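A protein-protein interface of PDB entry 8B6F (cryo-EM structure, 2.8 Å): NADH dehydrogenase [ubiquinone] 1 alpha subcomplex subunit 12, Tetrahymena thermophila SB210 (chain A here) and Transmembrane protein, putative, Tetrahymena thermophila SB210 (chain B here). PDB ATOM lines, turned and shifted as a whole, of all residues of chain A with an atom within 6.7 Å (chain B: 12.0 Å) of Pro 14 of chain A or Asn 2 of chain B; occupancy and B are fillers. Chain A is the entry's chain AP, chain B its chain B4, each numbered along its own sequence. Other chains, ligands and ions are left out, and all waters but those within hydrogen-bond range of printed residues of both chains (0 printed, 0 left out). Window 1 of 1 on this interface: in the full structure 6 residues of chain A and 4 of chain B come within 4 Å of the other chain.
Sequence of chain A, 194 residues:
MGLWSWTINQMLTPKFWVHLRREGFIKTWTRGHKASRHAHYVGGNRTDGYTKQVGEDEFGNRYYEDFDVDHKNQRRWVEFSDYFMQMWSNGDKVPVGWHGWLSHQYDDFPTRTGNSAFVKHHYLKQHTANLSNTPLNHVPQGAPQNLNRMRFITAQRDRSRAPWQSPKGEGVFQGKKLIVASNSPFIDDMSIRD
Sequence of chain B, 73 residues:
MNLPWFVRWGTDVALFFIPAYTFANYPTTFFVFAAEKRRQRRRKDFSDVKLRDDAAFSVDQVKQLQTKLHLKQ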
ATOM      1  N   GLN A  10       4.602  -0.392 -34.033  1.00  0.00           N
ATOM      2  CA  GLN A  10       4.370   1.047 -34.094  1.00  0.00           C
ATOM      3  C   GLN A  10       2.889   1.382 -34.189  1.00  0.00           C
ATOM      4  O   GLN A  10       2.463   2.428 -33.688  1.00  0.00           O
ATOM      5  CB  GLN A  10       5.120   1.658 -35.278  1.00  0.00           C
ATOM      6  CG  GLN A  10       6.625   1.685 -35.099  1.00  0.00           C
ATOM      7  CD  GLN A  10       7.051   2.545 -33.927  1.00  0.00           C
ATOM      8  OE1 GLN A  10       6.542   3.648 -33.738  1.00  0.00           O
ATOM      9  NE2 GLN A  10       7.980   2.037 -33.126  1.00  0.00           N
ATOM     10  N   MET A  11       2.092   0.521 -34.825  1.00  0.00           N
ATOM     11  CA  MET A  11       0.651   0.733 -34.855  1.00  0.00           C
ATOM     12  C   MET A  11      -0.002   0.405 -33.521  1.00  0.00           C
ATOM     13  O   MET A  11      -1.122   0.862 -33.266  1.00  0.00           O
ATOM     14  CB  MET A  11       0.016  -0.106 -35.965  1.00  0.00           C
ATOM     15  CG  MET A  11       0.378   0.360 -37.367  1.00  0.00           C
ATOM     16  SD  MET A  11      -0.555  -0.477 -38.662  1.00  0.00           S
ATOM     17  CE  MET A  11       0.019  -2.158 -38.460  1.00  0.00           C
ATOM     18  N   LEU A  12       0.661  -0.373 -32.670  1.00  0.00           N
ATOM     19  CA  LEU A  12       0.172  -0.654 -31.328  1.00  0.00           C
ATOM     20  C   LEU A  12       0.468   0.467 -30.340  1.00  0.00           C
ATOM     21  O   LEU A  12       0.338   0.255 -29.130  1.00  0.00           O
ATOM     22  CB  LEU A  12       0.776  -1.964 -30.815  1.00  0.00           C
ATOM     23  CG  LEU A  12       0.243  -3.253 -31.444  1.00  0.00           C
ATOM     24  CD1 LEU A  12       1.069  -4.444 -30.991  1.00  0.00           C
ATOM     25  CD2 LEU A  12      -1.223  -3.466 -31.101  1.00  0.00           C
ATOM     26  N   THR A  13       0.860   1.648 -30.820  1.00  0.00           N
ATOM     27  CA  THR A  13       1.184   2.770 -29.957  1.00  0.00           C
ATOM     28  C   THR A  13       0.121   3.860 -30.068  1.00  0.00           C
ATOM     29  O   THR A  13      -0.559   3.968 -31.092  1.00  0.00           O
ATOM     30  CB  THR A  13       2.551   3.368 -30.313  1.00  0.00           C
ATOM     31  OG1 THR A  13       2.590   3.684 -31.711  1.00  0.00           O
ATOM     32  CG2 THR A  13       3.662   2.389 -29.983  1.00  0.00           C
ATOM     33  N   PRO A  14      -0.049   4.685 -29.031  1.00  0.00           N
ATOM     34  CA  PRO A  14      -1.032   5.777 -29.126  1.00  0.00           C
ATOM     35  C   PRO A  14      -0.758   6.742 -30.262  1.00  0.00           C
ATOM     36  O   PRO A  14      -1.704   7.307 -30.822  1.00  0.00           O
ATOM     37  CB  PRO A  14      -0.920   6.468 -27.759  1.00  0.00           C
ATOM     38  CG  PRO A  14      -0.365   5.434 -26.852  1.00  0.00           C
ATOM     39  CD  PRO A  14       0.552   4.600 -27.690  1.00  0.00           C
ATOM     40  N   LYS A  15       0.510   6.953 -30.619  1.00  0.00           N
ATOM     41  CA  LYS A  15       0.830   7.920 -31.665  1.00  0.00           C
ATOM     42  C   LYS A  15       0.145   7.564 -32.978  1.00  0.00           C
ATOM     43  O   LYS A  15      -0.408   8.437 -33.654  1.00  0.00           O
ATOM     44  CB  LYS A  15       2.344   8.004 -31.859  1.00  0.00           C
ATOM     45  CG  LYS A  15       3.007   6.663 -32.138  1.00  0.00           C
ATOM     46  CD  LYS A  15       4.505   6.800 -32.339  1.00  0.00           C
ATOM     47  CE  LYS A  15       4.834   7.479 -33.653  1.00  0.00           C
ATOM     48  NZ  LYS A  15       6.294   7.426 -33.937  1.00  0.00           N
ATOM     49  N   PHE A  16       0.179   6.287 -33.361  1.00  0.00           N
ATOM     50  CA  PHE A  16      -0.434   5.886 -34.621  1.00  0.00           C
ATOM     51  C   PHE A  16      -1.929   6.167 -34.622  1.00  0.00           C
ATOM     52  O   PHE A  16      -2.476   6.657 -35.617  1.00  0.00           O
ATOM     53  CB  PHE A  16      -0.175   4.405 -34.884  1.00  0.00           C
ATOM     54  CG  PHE A  16      -0.998   3.839 -36.001  1.00  0.00           C
ATOM     55  CD1 PHE A  16      -0.677   4.106 -37.320  1.00  0.00           C
ATOM     56  CD2 PHE A  16      -2.091   3.034 -35.733  1.00  0.00           C
ATOM     57  CE1 PHE A  16      -1.432   3.586 -38.350  1.00  0.00           C
ATOM     58  CE2 PHE A  16      -2.852   2.512 -36.759  1.00  0.00           C
ATOM     59  CZ  PHE A  16      -2.520   2.787 -38.069  1.00  0.00           C
ATOM     60  N   TRP A  17      -2.609   5.866 -33.517  1.00  0.00           N
ATOM     61  CA  TRP A  17      -4.056   6.046 -33.476  1.00  0.00           C
ATOM     62  C   TRP A  17      -4.430   7.522 -33.519  1.00  0.00           C
ATOM     63  O   TRP A  17      -5.382   7.904 -34.210  1.00  0.00           O
ATOM     64  CB  TRP A  17      -4.626   5.368 -32.232  1.00  0.00           C
ATOM     65  CG  TRP A  17      -4.370   3.895 -32.223  1.00  0.00           C
ATOM     66  CD1 TRP A  17      -3.470   3.224 -31.447  1.00  0.00           C
ATOM     67  CD2 TRP A  17      -5.006   2.907 -33.045  1.00  0.00           C
ATOM     68  NE1 TRP A  17      -3.512   1.879 -31.728  1.00  0.00           N
ATOM     69  CE2 TRP A  17      -4.448   1.659 -32.705  1.00  0.00           C
ATOM     70  CE3 TRP A  17      -5.998   2.957 -34.030  1.00  0.00           C
ATOM     71  CZ2 TRP A  17      -4.845   0.470 -33.317  1.00  0.00           C
ATOM     72  CZ3 TRP A  17      -6.394   1.776 -34.637  1.00  0.00           C
ATOM     73  CH2 TRP A  17      -5.817   0.549 -34.278  1.00  0.00           C
ATOM     74  N   VAL A  18      -3.702   8.366 -32.790  1.00  0.00           N
ATOM     75  CA  VAL A  18      -3.974   9.800 -32.837  1.00  0.00           C
ATOM     76  C   VAL A  18      -3.724  10.338 -34.238  1.00  0.00           C
ATOM     77  O   VAL A  18      -4.509  11.134 -34.765  1.00  0.00           O
ATOM     78  CB  VAL A  18      -3.128  10.542 -31.787  1.00  0.00           C
ATOM     79  CG1 VAL A  18      -3.356  12.045 -31.876  1.00  0.00           C
ATOM     80  CG2 VAL A  18      -3.457  10.040 -30.392  1.00  0.00           C
ATOM     81  N   HIS A  19      -2.619   9.921 -34.861  1.00  0.00           N
ATOM     82  CA  HIS A  19      -2.311  10.387 -36.208  1.00  0.00           C
ATOM     83  C   HIS A  19      -3.375   9.940 -37.202  1.00  0.00           C
ATOM     84  O   HIS A  19      -3.793  10.716 -38.069  1.00  0.00           O
ATOM     85  CB  HIS A  19      -0.933   9.881 -36.634  1.00  0.00           C
ATOM     86  CG  HIS A  19      -0.295  10.709 -37.704  1.00  0.00           C
ATOM     87  ND1 HIS A  19      -0.689  10.654 -39.023  1.00  0.00           N
ATOM     88  CD2 HIS A  19       0.708  11.617 -37.649  1.00  0.00           C
ATOM     89  CE1 HIS A  19       0.042  11.492 -39.734  1.00  0.00           C
ATOM     90  NE2 HIS A  19       0.898  12.088 -38.925  1.00  0.00           N
ATOM     91  N   ARG A  21      -6.519   9.267 -36.501  1.00  0.00           N
ATOM     92  CA  ARG A  21      -7.749   9.997 -36.222  1.00  0.00           C
ATOM     93  C   ARG A  21      -7.717  11.394 -36.827  1.00  0.00           C
ATOM     94  O   ARG A  21      -8.715  11.854 -37.395  1.00  0.00           O
ATOM     95  CB  ARG A  21      -7.974  10.074 -34.714  1.00  0.00           C
ATOM     96  CG  ARG A  21      -9.330  10.628 -34.311  1.00  0.00           C
ATOM     97  CD  ARG A  21      -9.292  11.157 -32.888  1.00  0.00           C
ATOM     98  NE  ARG A  21      -8.699  10.195 -31.968  1.00  0.00           N
ATOM     99  CZ  ARG A  21      -8.389  10.456 -30.706  1.00  0.00           C
ATOM    100  NH1 ARG A  21      -8.600  11.649 -30.175  1.00  0.00           N
ATOM    101  NH2 ARG A  21      -7.851   9.498 -29.958  1.00  0.00           N
ATOM    102  N   THR A  47       6.510   7.517 -28.289  1.00  0.00           N
ATOM    103  CA  THR A  47       5.355   6.669 -28.561  1.00  0.00           C
ATOM    104  C   THR A  47       4.032   7.281 -28.126  1.00  0.00           C
ATOM    105  O   THR A  47       2.993   6.954 -28.707  1.00  0.00           O
ATOM    106  CB  THR A  47       5.515   5.313 -27.865  1.00  0.00           C
ATOM    107  OG1 THR A  47       5.548   5.501 -26.445  1.00  0.00           O
ATOM    108  CG2 THR A  47       6.797   4.630 -28.314  1.00  0.00           C
ATOM    109  N   ASP A  48       4.040   8.153 -27.118  1.00  0.00           N
ATOM    110  CA  ASP A  48       2.801   8.745 -26.625  1.00  0.00           C
ATOM    111  C   ASP A  48       2.219   9.781 -27.577  1.00  0.00           C
ATOM    112  O   ASP A  48       1.077  10.206 -27.375  1.00  0.00           O
ATOM    113  CB  ASP A  48       3.033   9.379 -25.252  1.00  0.00           C
ATOM    114  CG  ASP A  48       4.203  10.339 -25.244  1.00  0.00           C
ATOM    115  OD1 ASP A  48       5.143  10.132 -26.038  1.00  0.00           O
ATOM    116  OD2 ASP A  48       4.188  11.296 -24.440  1.00  0.00           O
ATOM    117  N   GLY A  49       2.964  10.197 -28.594  1.00  0.00           N
ATOM    118  CA  GLY A  49       2.462  11.165 -29.552  1.00  0.00           C
ATOM    119  C   GLY A  49       3.450  11.330 -30.681  1.00  0.00           C
ATOM    120  O   GLY A  49       4.584  10.849 -30.618  1.00  0.00           O
ATOM    121  N   TYR A  50       3.002  12.023 -31.723  1.00  0.00           N
ATOM    122  CA  TYR A  50       3.818  12.256 -32.905  1.00  0.00           C
ATOM    123  C   TYR A  50       4.312  13.696 -32.930  1.00  0.00           C
ATOM    124  O   TYR A  50       3.632  14.615 -32.468  1.00  0.00           O
ATOM    125  CB  TYR A  50       3.043  11.940 -34.190  1.00  0.00           C
ATOM    126  CG  TYR A  50       1.844  12.819 -34.448  1.00  0.00           C
ATOM    127  CD1 TYR A  50       0.597  12.492 -33.938  1.00  0.00           C
ATOM    128  CD2 TYR A  50       1.955  13.957 -35.231  1.00  0.00           C
ATOM    129  CE1 TYR A  50      -0.504  13.287 -34.185  1.00  0.00           C
ATOM    130  CE2 TYR A  50       0.861  14.758 -35.486  1.00  0.00           C
ATOM    131  CZ  TYR A  50      -0.366  14.418 -34.961  1.00  0.00           C
ATOM    132  OH  TYR A  50      -1.457  15.214 -35.211  1.00  0.00           O
ATOM    133  N   MET B   1      -3.783   3.713 -22.383  1.00  0.00           N
ATOM    134  CA  MET B   1      -3.909   3.280 -23.802  1.00  0.00           C
ATOM    135  C   MET B   1      -2.598   2.679 -24.296  1.00  0.00           C
ATOM    136  O   MET B   1      -2.593   1.777 -25.133  1.00  0.00           O
ATOM    137  CB  MET B   1      -4.317   4.461 -24.688  1.00  0.00           C
ATOM    138  CG  MET B   1      -4.529   4.090 -26.149  1.00  0.00           C
ATOM    139  SD  MET B   1      -5.095   5.476 -27.151  1.00  0.00           S
ATOM    140  CE  MET B   1      -5.226   4.696 -28.757  1.00  0.00           C
ATOM    141  N   ASN B   2      -1.487   3.183 -23.769  1.00  0.00           N
ATOM    142  CA  ASN B   2      -0.177   2.709 -24.182  1.00  0.00           C
ATOM    143  C   ASN B   2       0.056   1.282 -23.696  1.00  0.00           C
ATOM    144  O   ASN B   2      -0.591   0.796 -22.763  1.00  0.00           O
ATOM    145  CB  ASN B   2       0.921   3.626 -23.644  1.00  0.00           C
ATOM    146  CG  ASN B   2       0.929   3.701 -22.132  1.00  0.00           C
ATOM    147  OD1 ASN B   2      -0.112   3.577 -21.488  1.00  0.00           O
ATOM    148  ND2 ASN B   2       2.108   3.902 -21.556  1.00  0.00           N
ATOM    149  N   LEU B   3       0.998   0.609 -24.348  1.00  0.00           N
ATOM    150  CA  LEU B   3       1.389  -0.747 -24.008  1.00  0.00           C
ATOM    151  C   LEU B   3       2.893  -0.802 -23.787  1.00  0.00           C
ATOM    152  O   LEU B   3       3.639  -0.012 -24.374  1.00  0.00           O
ATOM    153  CB  LEU B   3       0.999  -1.737 -25.118  1.00  0.00           C
ATOM    154  CG  LEU B   3      -0.500  -1.952 -25.355  1.00  0.00           C
ATOM    155  CD1 LEU B   3      -0.730  -2.839 -26.567  1.00  0.00           C
ATOM    156  CD2 LEU B   3      -1.165  -2.555 -24.129  1.00  0.00           C
ATOM    157  N   PRO B   4       3.366  -1.719 -22.944  1.00  0.00           N
ATOM    158  CA  PRO B   4       4.809  -1.808 -22.692  1.00  0.00           C
ATOM    159  C   PRO B   4       5.578  -2.216 -23.938  1.00  0.00           C
ATOM    160  O   PRO B   4       5.081  -2.949 -24.796  1.00  0.00           O
ATOM    161  CB  PRO B   4       4.917  -2.877 -21.598  1.00  0.00           C
ATOM    162  CG  PRO B   4       3.575  -2.944 -20.981  1.00  0.00           C
ATOM    163  CD  PRO B   4       2.602  -2.624 -22.069  1.00  0.00           C
ATOM    164  N   TRP B   5       6.814  -1.722 -24.028  1.00  0.00           N
ATOM    165  CA  TRP B   5       7.682  -2.092 -25.140  1.00  0.00           C
ATOM    166  C   TRP B   5       7.900  -3.598 -25.189  1.00  0.00           C
ATOM    167  O   TRP B   5       7.939  -4.191 -26.272  1.00  0.00           O
ATOM    168  CB  TRP B   5       9.023  -1.365 -25.026  1.00  0.00           C
ATOM    169  CG  TRP B   5       9.863  -1.825 -23.873  1.00  0.00           C
ATOM    170  CD1 TRP B   5       9.947  -1.248 -22.641  1.00  0.00           C
ATOM    171  CD2 TRP B   5      10.740  -2.960 -23.845  1.00  0.00           C
ATOM    172  NE1 TRP B   5      10.820  -1.950 -21.848  1.00  0.00           N
ATOM    173  CE2 TRP B   5      11.320  -3.006 -22.564  1.00  0.00           C
ATOM    174  CE3 TRP B   5      11.089  -3.941 -24.780  1.00  0.00           C
ATOM    175  CZ2 TRP B   5      12.229  -3.994 -22.192  1.00  0.00           C
ATOM    176  CZ3 TRP B   5      11.992  -4.921 -24.409  1.00  0.00           C
ATOM    177  CH2 TRP B   5      12.553  -4.940 -23.125  1.00  0.00           C
ATOM    178  N   PHE B   6       8.047  -4.236 -24.026  1.00  0.00           N
ATOM    179  CA  PHE B   6       8.241  -5.681 -24.010  1.00  0.00           C
ATOM    180  C   PHE B   6       6.975  -6.416 -24.428  1.00  0.00           C
ATOM    181  O   PHE B   6       7.060  -7.500 -25.015  1.00  0.00           O
ATOM    182  CB  PHE B   6       8.712  -6.144 -22.629  1.00  0.00           C
ATOM    183  CG  PHE B   6       7.837  -5.693 -21.494  1.00  0.00           C
ATOM    184  CD1 PHE B   6       6.693  -6.394 -21.162  1.00  0.00           C
ATOM    185  CD2 PHE B   6       8.182  -4.584 -20.737  1.00  0.00           C
ATOM    186  CE1 PHE B   6       5.896  -5.989 -20.109  1.00  0.00           C
ATOM    187  CE2 PHE B   6       7.392  -4.173 -19.684  1.00  0.00           C
ATOM    188  CZ  PHE B   6       6.247  -4.875 -19.368  1.00  0.00           C
ATOM    189  N   VAL B   7       5.799  -5.859 -24.138  1.00  0.00           N
ATOM    190  CA  VAL B   7       4.564  -6.461 -24.630  1.00  0.00           C
ATOM    191  C   VAL B   7       4.533  -6.422 -26.153  1.00  0.00           C
ATOM    192  O   VAL B   7       4.187  -7.410 -26.811  1.00  0.00           O
ATOM    193  CB  VAL B   7       3.340  -5.750 -24.022  1.00  0.00           C
ATOM    194  CG1 VAL B   7       2.056  -6.153 -24.742  1.00  0.00           C
ATOM    195  CG2 VAL B   7       3.236  -6.063 -22.541  1.00  0.00           C
ATOM    196  N   ARG B   8       4.887  -5.275 -26.740  1.00  0.00           N
ATOM    197  CA  ARG B   8       4.901  -5.170 -28.196  1.00  0.00           C
ATOM    198  C   ARG B   8       5.948  -6.094 -28.806  1.00  0.00           C
ATOM    199  O   ARG B   8       5.702  -6.727 -29.838  1.00  0.00           O
ATOM    200  CB  ARG B   8       5.148  -3.722 -28.614  1.00  0.00           C
ATOM    201  CG  ARG B   8       3.966  -2.802 -28.343  1.00  0.00           C
ATOM    202  CD  ARG B   8       4.425  -1.419 -27.919  1.00  0.00           C
ATOM    203  NE  ARG B   8       5.327  -0.817 -28.893  1.00  0.00           N
ATOM    204  CZ  ARG B   8       6.000   0.308 -28.693  1.00  0.00           C
ATOM    205  NH1 ARG B   8       5.899   0.982 -27.560  1.00  0.00           N
ATOM    206  NH2 ARG B   8       6.800   0.763 -29.652  1.00  0.00           N
ATOM    207  N   TRP B   9       7.129  -6.174 -28.190  1.00  0.00           N
ATOM    208  CA  TRP B   9       8.170  -7.059 -28.703  1.00  0.00           C
ATOM    209  C   TRP B   9       7.745  -8.517 -28.599  1.00  0.00           C
ATOM    210  O   TRP B   9       8.009  -9.313 -29.507  1.00  0.00           O
ATOM    211  CB  TRP B   9       9.484  -6.829 -27.960  1.00  0.00           C
ATOM    212  CG  TRP B   9      10.613  -7.652 -28.503  1.00  0.00           C
ATOM    213  CD1 TRP B   9      11.019  -7.728 -29.803  1.00  0.00           C
ATOM    214  CD2 TRP B   9      11.484  -8.512 -27.760  1.00  0.00           C
ATOM    215  NE1 TRP B   9      12.088  -8.583 -29.914  1.00  0.00           N
ATOM    216  CE2 TRP B   9      12.393  -9.078 -28.675  1.00  0.00           C
ATOM    217  CE3 TRP B   9      11.583  -8.859 -26.409  1.00  0.00           C
ATOM    218  CZ2 TRP B   9      13.389  -9.972 -28.283  1.00  0.00           C
ATOM    219  CZ3 TRP B   9      12.571  -9.747 -26.020  1.00  0.00           C
ATOM    220  CH2 TRP B   9      13.462 -10.293 -26.955  1.00  0.00           C
ATOM    221  N   THR B  11       4.682  -9.500 -28.786  1.00  0.00           N
ATOM    222  CA  THR B  11       3.721  -9.672 -29.868  1.00  0.00           C
ATOM    223  C   THR B  11       4.434  -9.981 -31.178  1.00  0.00           C
ATOM    224  O   THR B  11       4.020 -10.878 -31.921  1.00  0.00           O
ATOM    225  CB  THR B  11       2.857  -8.418 -30.008  1.00  0.00           C
ATOM    226  OG1 THR B  11       2.122  -8.203 -28.797  1.00  0.00           O
ATOM    227  CG2 THR B  11       1.875  -8.560 -31.165  1.00  0.00           C
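O of Met 11 of chain A lies within hydrogen-bond range of NE1 of Trp 17 of chain A, 3.0 Å away. The backbone NH (N) of Lys 15 of chain A lies within hydrogen-bond range of the backbone carbonyl oxygen (O) of Thr 47 of chain A (3.1 Å).
Among the printed residues, pairs that only touch across the chains: Gln 10 of chain A with Arg 8 of chain B (3.9 Å), Thr 13 of chain A with Arg 8 of chain B (3.4 Å), Pro 14 of chain A with Asn 2 of chain B (3.8 Å), Trp 17 of chain A with Met 1 of chain B (3.5 Å) and Thr 47 of chain A with Arg 8 of chain B (3.8 Å).
Of the printed residues of chain B, Gln 10 of chain A touches Arg 8 (3.9 Å). Of the printed residues of chain B, Pro 14 of chain A touches Asn 2 (3.8 Å). Of the printed residues of chain B, Trp 17 of chain A touches Met 1. Val 18 of chain A touches none of the printed residues of chain B. Of chain B, only Arg 8 (3.8 Å) comes within 4 Å of Thr 47 of chain A. No residue of chain B comes within 4 Å of Gly 49 of chain A. Printed residues of chain A within 4 Å of Met 1 of chain B: Trp 17 (3.5 Å). Asn 2 of chain B touches just one residue of chain A: Pro 14 (3.8 Å). Phe 6 of chain B touches none of the printed residues of chain A. Printed residues of chain A within 4 Å of Arg 8 of chain B: Gln 10 (3.9 Å), Thr 13 (3.4 Å) and Thr 47 (3.8 Å). The nearest residue of chain B that does not touch Pro 14 of chain A is Met 1 of chain B (4.3 Å).
Printed residues of chain A that touch a printed residue of chain B: Gln 10, Thr 13, Pro 14, Trp 17 and Thr 47. Of the 10 printed residues of chain B, 3 touch a printed residue of chain A. Hydrophobic or aromatic side chains of chain B that line the printed part of chain A: Met 1. Among the printed residues, 5 pairs touch across the chains.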
